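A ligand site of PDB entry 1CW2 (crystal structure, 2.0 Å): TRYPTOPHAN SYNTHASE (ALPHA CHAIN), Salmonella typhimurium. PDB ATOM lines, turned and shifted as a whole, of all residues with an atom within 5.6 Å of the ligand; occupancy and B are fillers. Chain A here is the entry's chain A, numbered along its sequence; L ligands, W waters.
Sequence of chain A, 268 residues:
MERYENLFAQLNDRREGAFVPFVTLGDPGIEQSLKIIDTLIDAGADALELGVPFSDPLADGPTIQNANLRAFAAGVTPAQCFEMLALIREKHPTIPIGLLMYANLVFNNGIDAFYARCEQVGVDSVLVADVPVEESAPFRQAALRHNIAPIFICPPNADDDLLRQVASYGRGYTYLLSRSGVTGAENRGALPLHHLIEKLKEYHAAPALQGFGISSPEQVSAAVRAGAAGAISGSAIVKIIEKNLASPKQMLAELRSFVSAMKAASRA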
ATOM      1  N   PHE A  22       1.993 -16.640   6.418  1.00  0.00           N
ATOM      2  CA  PHE A  22       2.186 -17.074   7.790  1.00  0.00           C
ATOM      3  C   PHE A  22       3.216 -16.195   8.495  1.00  0.00           C
ATOM      4  O   PHE A  22       4.203 -15.782   7.879  1.00  0.00           O
ATOM      5  CB  PHE A  22       2.679 -18.532   7.847  1.00  0.00           C
ATOM      6  CG  PHE A  22       3.165 -18.949   9.226  1.00  0.00           C
ATOM      7  CD1 PHE A  22       4.442 -18.587   9.671  1.00  0.00           C
ATOM      8  CD2 PHE A  22       2.321 -19.645  10.095  1.00  0.00           C
ATOM      9  CE1 PHE A  22       4.862 -18.906  10.948  1.00  0.00           C
ATOM     10  CE2 PHE A  22       2.742 -19.976  11.380  1.00  0.00           C
ATOM     11  CZ  PHE A  22       4.011 -19.601  11.809  1.00  0.00           C
ATOM     12  N   GLU A  49      -2.505 -17.212   8.727  1.00  0.00           N
ATOM     13  CA  GLU A  49      -2.089 -18.398   9.481  1.00  0.00           C
ATOM     14  C   GLU A  49      -1.086 -17.801  10.468  1.00  0.00           C
ATOM     15  O   GLU A  49      -0.036 -17.289  10.065  1.00  0.00           O
ATOM     16  CB  GLU A  49      -1.428 -19.430   8.569  1.00  0.00           C
ATOM     17  CG  GLU A  49      -1.366 -20.851   9.160  1.00  0.00           C
ATOM     18  CD  GLU A  49      -2.710 -21.445   9.539  1.00  0.00           C
ATOM     19  OE1 GLU A  49      -3.707 -21.279   8.796  1.00  0.00           O
ATOM     20  OE2 GLU A  49      -2.768 -22.124  10.586  1.00  0.00           O
ATOM     21  N   ALA A  59       8.067 -29.091  14.027  1.00  0.00           N
ATOM     22  CA  ALA A  59       7.619 -29.277  12.648  1.00  0.00           C
ATOM     23  C   ALA A  59       8.103 -28.101  11.805  1.00  0.00           C
ATOM     24  O   ALA A  59       7.777 -27.996  10.617  1.00  0.00           O
ATOM     25  CB  ALA A  59       6.096 -29.386  12.597  1.00  0.00           C
ATOM     26  N   ASP A  60       8.947 -27.261  12.398  1.00  0.00           N
ATOM     27  CA  ASP A  60       9.454 -26.079  11.734  1.00  0.00           C
ATOM     28  C   ASP A  60      10.955 -26.044  11.482  1.00  0.00           C
ATOM     29  O   ASP A  60      11.745 -26.407  12.348  1.00  0.00           O
ATOM     30  CB  ASP A  60       9.053 -24.827  12.540  1.00  0.00           C
ATOM     31  CG  ASP A  60       7.563 -24.501  12.426  1.00  0.00           C
ATOM     32  OD1 ASP A  60       7.098 -24.246  11.298  1.00  0.00           O
ATOM     33  OD2 ASP A  60       6.870 -24.491  13.460  1.00  0.00           O
ATOM     34  N   ILE A  64      11.399 -20.360  10.695  1.00  0.00           N
ATOM     35  CA  ILE A  64      10.317 -20.215  11.658  1.00  0.00           C
ATOM     36  C   ILE A  64      10.784 -20.506  13.100  1.00  0.00           C
ATOM     37  O   ILE A  64      10.243 -19.967  14.067  1.00  0.00           O
ATOM     38  CB  ILE A  64       9.095 -21.068  11.243  1.00  0.00           C
ATOM     39  CG1 ILE A  64       8.504 -20.502   9.947  1.00  0.00           C
ATOM     40  CG2 ILE A  64       8.021 -21.030  12.325  1.00  0.00           C
ATOM     41  CD1 ILE A  64       7.369 -21.328   9.367  1.00  0.00           C
ATOM     42  N   LEU A 100      -1.599 -21.703  14.343  1.00  0.00           N
ATOM     43  CA  LEU A 100      -0.697 -22.851  14.187  1.00  0.00           C
ATOM     44  C   LEU A 100      -0.289 -23.076  15.643  1.00  0.00           C
ATOM     45  O   LEU A 100       0.374 -22.210  16.242  1.00  0.00           O
ATOM     46  CB  LEU A 100       0.533 -22.514  13.345  1.00  0.00           C
ATOM     47  CG  LEU A 100       1.542 -23.660  13.119  1.00  0.00           C
ATOM     48  CD1 LEU A 100       2.509 -23.836  14.301  1.00  0.00           C
ATOM     49  CD2 LEU A 100       0.812 -24.963  12.842  1.00  0.00           C
ATOM     50  N   TYR A 102       1.018 -26.003  18.892  1.00  0.00           N
ATOM     51  CA  TYR A 102       1.661 -27.275  19.234  1.00  0.00           C
ATOM     52  C   TYR A 102       0.769 -27.743  20.385  1.00  0.00           C
ATOM     53  O   TYR A 102       0.180 -26.914  21.093  1.00  0.00           O
ATOM     54  CB  TYR A 102       3.127 -27.115  19.604  1.00  0.00           C
ATOM     55  CG  TYR A 102       4.000 -27.059  18.367  1.00  0.00           C
ATOM     56  CD1 TYR A 102       4.490 -28.221  17.791  1.00  0.00           C
ATOM     57  CD2 TYR A 102       4.274 -25.841  17.755  1.00  0.00           C
ATOM     58  CE1 TYR A 102       5.255 -28.176  16.610  1.00  0.00           C
ATOM     59  CE2 TYR A 102       5.033 -25.772  16.572  1.00  0.00           C
ATOM     60  CZ  TYR A 102       5.518 -26.943  16.010  1.00  0.00           C
ATOM     61  OH  TYR A 102       6.241 -26.904  14.848  1.00  0.00           O
ATOM     62  N   LEU A 127      -4.916 -25.540  13.867  1.00  0.00           N
ATOM     63  CA  LEU A 127      -4.141 -26.669  13.374  1.00  0.00           C
ATOM     64  C   LEU A 127      -3.148 -26.931  14.498  1.00  0.00           C
ATOM     65  O   LEU A 127      -2.441 -26.011  14.935  1.00  0.00           O
ATOM     66  CB  LEU A 127      -3.360 -26.280  12.105  1.00  0.00           C
ATOM     67  CG  LEU A 127      -2.150 -27.144  11.680  1.00  0.00           C
ATOM     68  CD1 LEU A 127      -2.575 -28.593  11.448  1.00  0.00           C
ATOM     69  CD2 LEU A 127      -1.489 -26.570  10.413  1.00  0.00           C
ATOM     70  N   ALA A 129       0.007 -28.880  15.092  1.00  0.00           N
ATOM     71  CA  ALA A 129       1.031 -29.576  14.325  1.00  0.00           C
ATOM     72  C   ALA A 129       1.419 -30.995  14.762  1.00  0.00           C
ATOM     73  O   ALA A 129       1.676 -31.841  13.896  1.00  0.00           O
ATOM     74  CB  ALA A 129       2.274 -28.692  14.157  1.00  0.00           C
ATOM     75  N   ILE A 153      -4.070 -32.316   8.438  1.00  0.00           N
ATOM     76  CA  ILE A 153      -3.025 -32.373   7.426  1.00  0.00           C
ATOM     77  C   ILE A 153      -3.119 -33.642   6.577  1.00  0.00           C
ATOM     78  O   ILE A 153      -3.260 -34.752   7.101  1.00  0.00           O
ATOM     79  CB  ILE A 153      -1.616 -32.217   8.062  1.00  0.00           C
ATOM     80  CG1 ILE A 153      -1.433 -30.766   8.524  1.00  0.00           C
ATOM     81  CG2 ILE A 153      -0.514 -32.636   7.087  1.00  0.00           C
ATOM     82  CD1 ILE A 153      -0.032 -30.397   8.978  1.00  0.00           C
ATOM     83  N   TYR A 173     -10.619 -25.580   5.911  1.00  0.00           N
ATOM     84  CA  TYR A 173      -9.786 -25.913   4.755  1.00  0.00           C
ATOM     85  C   TYR A 173      -9.028 -27.197   5.107  1.00  0.00           C
ATOM     86  O   TYR A 173      -8.983 -27.591   6.281  1.00  0.00           O
ATOM     87  CB  TYR A 173      -8.820 -24.769   4.383  1.00  0.00           C
ATOM     88  CG  TYR A 173      -7.640 -24.540   5.325  1.00  0.00           C
ATOM     89  CD1 TYR A 173      -6.423 -25.187   5.123  1.00  0.00           C
ATOM     90  CD2 TYR A 173      -7.737 -23.643   6.392  1.00  0.00           C
ATOM     91  CE1 TYR A 173      -5.331 -24.959   5.952  1.00  0.00           C
ATOM     92  CE2 TYR A 173      -6.648 -23.403   7.227  1.00  0.00           C
ATOM     93  CZ  TYR A 173      -5.447 -24.055   7.010  1.00  0.00           C
ATOM     94  OH  TYR A 173      -4.350 -23.819   7.811  1.00  0.00           O
ATOM     95  N   TYR A 175      -5.428 -29.013   4.889  1.00  0.00           N
ATOM     96  CA  TYR A 175      -4.035 -28.614   4.730  1.00  0.00           C
ATOM     97  C   TYR A 175      -3.314 -29.626   3.829  1.00  0.00           C
ATOM     98  O   TYR A 175      -2.998 -30.729   4.280  1.00  0.00           O
ATOM     99  CB  TYR A 175      -3.350 -28.529   6.090  1.00  0.00           C
ATOM    100  CG  TYR A 175      -2.134 -27.631   6.104  1.00  0.00           C
ATOM    101  CD1 TYR A 175      -0.978 -27.979   5.407  1.00  0.00           C
ATOM    102  CD2 TYR A 175      -2.134 -26.426   6.814  1.00  0.00           C
ATOM    103  CE1 TYR A 175       0.148 -27.164   5.404  1.00  0.00           C
ATOM    104  CE2 TYR A 175      -1.023 -25.606   6.825  1.00  0.00           C
ATOM    105  CZ  TYR A 175       0.124 -25.982   6.114  1.00  0.00           C
ATOM    106  OH  TYR A 175       1.259 -25.182   6.113  1.00  0.00           O
ATOM    107  N   ARG A 179       5.022 -31.567   0.583  1.00  0.00           N
ATOM    108  CA  ARG A 179       6.307 -32.185   0.896  1.00  0.00           C
ATOM    109  C   ARG A 179       6.403 -32.925   2.235  1.00  0.00           C
ATOM    110  O   ARG A 179       5.661 -32.664   3.181  1.00  0.00           O
ATOM    111  CB  ARG A 179       7.322 -31.027   0.946  1.00  0.00           C
ATOM    112  CG  ARG A 179       8.749 -31.409   0.859  1.00  0.00           C
ATOM    113  CD  ARG A 179       9.675 -30.226   0.581  1.00  0.00           C
ATOM    114  NE  ARG A 179       9.440 -28.975   1.307  1.00  0.00           N
ATOM    115  CZ  ARG A 179       9.437 -28.812   2.633  1.00  0.00           C
ATOM    116  NH1 ARG A 179       9.625 -29.836   3.468  1.00  0.00           N
ATOM    117  NH2 ARG A 179       9.373 -27.589   3.124  1.00  0.00           N
ATOM    118  N   VAL A 182      10.071 -30.639   7.200  1.00  0.00           N
ATOM    119  CA  VAL A 182       9.625 -29.488   7.987  1.00  0.00           C
ATOM    120  C   VAL A 182       9.419 -28.212   7.144  1.00  0.00           C
ATOM    121  O   VAL A 182       9.701 -28.210   5.929  1.00  0.00           O
ATOM    122  CB  VAL A 182      10.629 -29.156   9.123  1.00  0.00           C
ATOM    123  CG1 VAL A 182      10.756 -30.335  10.068  1.00  0.00           C
ATOM    124  CG2 VAL A 182      11.977 -28.781   8.550  1.00  0.00           C
ATOM    125  N   THR A 183       8.911 -27.149   7.760  1.00  0.00           N
ATOM    126  CA  THR A 183       8.680 -25.881   7.065  1.00  0.00           C
ATOM    127  C   THR A 183      10.006 -25.271   6.613  1.00  0.00           C
ATOM    128  O   THR A 183      11.024 -25.371   7.319  1.00  0.00           O
ATOM    129  CB  THR A 183       7.947 -24.843   7.956  1.00  0.00           C
ATOM    130  OG1 THR A 183       8.768 -24.517   9.079  1.00  0.00           O
ATOM    131  CG2 THR A 183       6.616 -25.397   8.441  1.00  0.00           C
ATOM    132  N   GLY A 184       9.999 -24.634   5.449  1.00  0.00           N
ATOM    133  CA  GLY A 184      11.218 -24.017   4.954  1.00  0.00           C
ATOM    134  C   GLY A 184      11.124 -23.708   3.482  1.00  0.00           C
ATOM    135  O   GLY A 184      10.750 -24.581   2.691  1.00  0.00           O
ATOM    136  N   ALA A 185      11.417 -22.459   3.111  1.00  0.00           N
ATOM    137  CA  ALA A 185      11.377 -22.030   1.707  1.00  0.00           C
ATOM    138  C   ALA A 185      12.608 -22.567   0.990  1.00  0.00           C
ATOM    139  O   ALA A 185      12.739 -22.443  -0.228  1.00  0.00           O
ATOM    140  CB  ALA A 185      11.345 -20.501   1.631  1.00  0.00           C
ATOM    141  N   GLY A 211       0.509 -26.181   1.396  1.00  0.00           N
ATOM    142  CA  GLY A 211       1.516 -25.568   2.255  1.00  0.00           C
ATOM    143  C   GLY A 211       2.832 -26.332   2.294  1.00  0.00           C
ATOM    144  O   GLY A 211       2.828 -27.563   2.181  1.00  0.00           O
ATOM    145  N   PHE A 212       3.914 -25.591   2.541  1.00  0.00           N
ATOM    146  CA  PHE A 212       5.308 -26.063   2.613  1.00  0.00           C
ATOM    147  C   PHE A 212       6.073 -25.808   1.307  1.00  0.00           C
ATOM    148  O   PHE A 212       5.697 -26.313   0.227  1.00  0.00           O
ATOM    149  CB  PHE A 212       5.426 -27.554   2.971  1.00  0.00           C
ATOM    150  CG  PHE A 212       5.269 -27.842   4.451  1.00  0.00           C
ATOM    151  CD1 PHE A 212       6.054 -28.830   5.059  1.00  0.00           C
ATOM    152  CD2 PHE A 212       4.331 -27.158   5.225  1.00  0.00           C
ATOM    153  CE1 PHE A 212       5.912 -29.128   6.420  1.00  0.00           C
ATOM    154  CE2 PHE A 212       4.183 -27.453   6.579  1.00  0.00           C
ATOM    155  CZ  PHE A 212       4.975 -28.444   7.181  1.00  0.00           C
ATOM    156  N   GLY A 213       7.139 -25.021   1.423  1.00  0.00           N
ATOM    157  CA  GLY A 213       7.997 -24.700   0.284  1.00  0.00           C
ATOM    158  C   GLY A 213       7.528 -23.682  -0.735  1.00  0.00           C
ATOM    159  O   GLY A 213       8.267 -23.365  -1.677  1.00  0.00           O
ATOM    160  N   ILE A 214       6.319 -23.145  -0.570  1.00  0.00           N
ATOM    161  CA  ILE A 214       5.780 -22.152  -1.514  1.00  0.00           C
ATOM    162  C   ILE A 214       6.457 -20.799  -1.287  1.00  0.00           C
ATOM    163  O   ILE A 214       6.200 -20.141  -0.276  1.00  0.00           O
ATOM    164  CB  ILE A 214       4.248 -21.985  -1.325  1.00  0.00           C
ATOM    165  CG1 ILE A 214       3.522 -23.327  -1.393  1.00  0.00           C
ATOM    166  CG2 ILE A 214       3.682 -20.983  -2.350  1.00  0.00           C
ATOM    167  CD1 ILE A 214       3.505 -23.974  -2.744  1.00  0.00           C
ATOM    168  N   ILE A 232      -0.372 -21.558   1.028  1.00  0.00           N
ATOM    169  CA  ILE A 232       0.132 -20.937   2.261  1.00  0.00           C
ATOM    170  C   ILE A 232       1.650 -20.713   2.100  1.00  0.00           C
ATOM    171  O   ILE A 232       2.356 -21.571   1.566  1.00  0.00           O
ATOM    172  CB  ILE A 232      -0.117 -21.871   3.506  1.00  0.00           C
ATOM    173  CG1 ILE A 232      -1.617 -22.002   3.771  1.00  0.00           C
ATOM    174  CG2 ILE A 232       0.619 -21.337   4.754  1.00  0.00           C
ATOM    175  CD1 ILE A 232      -2.005 -23.203   4.622  1.00  0.00           C
ATOM    176  N   SER A 233       2.151 -19.555   2.530  1.00  0.00           N
ATOM    177  CA  SER A 233       3.574 -19.241   2.442  1.00  0.00           C
ATOM    178  C   SER A 233       4.073 -18.669   3.769  1.00  0.00           C
ATOM    179  O   SER A 233       3.632 -17.583   4.183  1.00  0.00           O
ATOM    180  CB  SER A 233       3.825 -18.230   1.320  1.00  0.00           C
ATOM    181  OG  SER A 233       5.204 -17.920   1.201  1.00  0.00           O
ATOM    182  N   GLY A 234       5.027 -19.346   4.394  1.00  0.00           N
ATOM    183  CA  GLY A 234       5.553 -18.893   5.680  1.00  0.00           C
ATOM    184  C   GLY A 234       6.997 -18.411   5.727  1.00  0.00           C
ATOM    185  O   GLY A 234       7.243 -17.237   5.946  1.00  0.00           O
ATOM    186  N   SER A 235       7.940 -19.309   5.490  1.00  0.00           N
ATOM    187  CA  SER A 235       9.369 -18.950   5.527  1.00  0.00           C
ATOM    188  C   SER A 235       9.749 -17.791   4.592  1.00  0.00           C
ATOM    189  O   SER A 235      10.597 -16.959   4.945  1.00  0.00           O
ATOM    190  CB  SER A 235      10.236 -20.184   5.245  1.00  0.00           C
ATOM    191  OG  SER A 235       9.962 -21.222   6.182  1.00  0.00           O
ATOM    192  N   ALA A 236       9.126 -17.745   3.414  1.00  0.00           N
ATOM    193  CA  ALA A 236       9.401 -16.664   2.476  1.00  0.00           C
ATOM    194  C   ALA A 236       8.985 -15.336   3.106  1.00  0.00           C
ATOM    195  O   ALA A 236       9.641 -14.305   2.908  1.00  0.00           O
ATOM    196  CB  ALA A 236       8.656 -16.896   1.176  1.00  0.00           C
HETATM  197  O1  LIG L   1       6.416 -21.830   3.472  1.00  0.00           O
HETATM  198  O2  LIG L   1       7.621 -23.879   3.926  1.00  0.00           O
HETATM  199  O3  LIG L   1       0.898 -23.783   8.284  1.00  0.00           O
HETATM  200  C1  LIG L   1       1.865 -25.938   9.458  1.00  0.00           C
HETATM  201  C2  LIG L   1       2.570 -24.794   9.840  1.00  0.00           C
HETATM  202  C3  LIG L   1       3.761 -24.905  10.602  1.00  0.00           C
HETATM  203  C4  LIG L   1       4.234 -26.176  10.974  1.00  0.00           C
HETATM  204  C5  LIG L   1       3.519 -27.327  10.585  1.00  0.00           C
HETATM  205  C6  LIG L   1       2.338 -27.209   9.830  1.00  0.00           C
HETATM  206  O4  LIG L   1       4.465 -23.803  10.986  1.00  0.00           O
HETATM  207  S1  LIG L   1       1.964 -23.175   9.368  1.00  0.00           S
HETATM  208  C7  LIG L   1       3.336 -22.369   8.490  1.00  0.00           C
HETATM  209  C8  LIG L   1       3.783 -23.230   7.312  1.00  0.00           C
HETATM  210  C9  LIG L   1       4.941 -22.575   6.576  1.00  0.00           C
HETATM  211  C10 LIG L   1       5.392 -23.448   5.392  1.00  0.00           C
HETATM  212  P1  LIG L   1       6.769 -22.813   4.580  1.00  0.00           P
HETATM  213  O5  LIG L   1       7.722 -22.050   5.484  1.00  0.00           O
HETATM  214  O   HOH W   1       7.767 -19.924   2.222  1.00  0.00           O
HETATM  215  O   HOH W   2       4.725 -22.942   1.857  1.00  0.00           O
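OD1 of Asp 60 is in hydrogen-bond range of OG1 of Thr 183, at 2.8 Å.
NH2 of Arg 179 lies within hydrogen-bond range of O of Gly 184, 3.3 Å away.
The backbone NH of Gly 184 sits close to the side-chain hydroxyl of Ser 235 (3.5 Å).
The backbone NH of Ala 59 is in hydrogen-bond range of the side-chain hydroxyl of Tyr 102 (3.0 Å).
The side-chain carboxylate of Glu 49 is in hydrogen-bond range of the side-chain hydroxyl of Tyr 173 (2.8 Å).
The backbone NH (N) of Phe 22 lies within hydrogen-bond range of the backbone carbonyl oxygen (O) of Ser 233 (2.9 Å).
O of Ala 59 is in hydrogen-bond range of N of Thr 183 (3.2 Å).
The backbone carbonyl oxygen (O) of Ile 214 is in hydrogen-bond range of the side-chain hydroxyl (OG) of Ser 233, at 2.8 Å.
OD1 of Asp 60 is in hydrogen-bond range of O4 of the ligand, 2.7 Å away.
An oxygen (O3) of the ligand is in hydrogen-bond range of the side-chain hydroxyl (OH) of Tyr 175 (2.6 Å).
OG of Ser 235 lies within hydrogen-bond range of O5 of the ligand, at 2.5 Å.
An oxygen (O2) of the ligand sits at hydrogen-bond distance from the backbone NH (N) of Gly 184 (2.9 Å).
N of Ser 235 is in hydrogen-bond range of O5 of the ligand.
N of Gly 213 sits at hydrogen-bond distance from O2 of the ligand (2.8 Å).
N of Gly 234 sits at hydrogen-bond distance from O1 of the ligand (3.0 Å).
Water W1 lies within hydrogen-bond range of an oxygen (O1) of the ligand (2.6 Å), the backbone NH of Ala 236 (2.8 Å), the backbone carbonyl oxygen of Ile 214 (3.0 Å), the backbone NH of Ser 235 (3.3 Å) and the side-chain hydroxyl of Ser 233 (3.4 Å).
Phe 22 touches the ligand.
Glu 49 touches the ligand (CG to O3, 3.8 Å).
CB of Ala 59 touches C5 of the ligand, 3.9 Å away.
Ile 64 touches the ligand (CD1 to C9, 3.9 Å).
Leu 100 touches the ligand (CD2 to C2, 3.5 Å).
Leu 127 touches the ligand (CD2 to C1, 3.5 Å).
Thr 183 touches the ligand (CG2 to C4, 3.6 Å).
Phe 212 touches the ligand.
C of Ser 233 touches O1 of the ligand, at 3.9 Å.
Of the 26 residues printed, 15 come within 4 Å of the ligand.
The nearest printed residue that does not touch the ligand is Ala 129 (4.02 Å).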
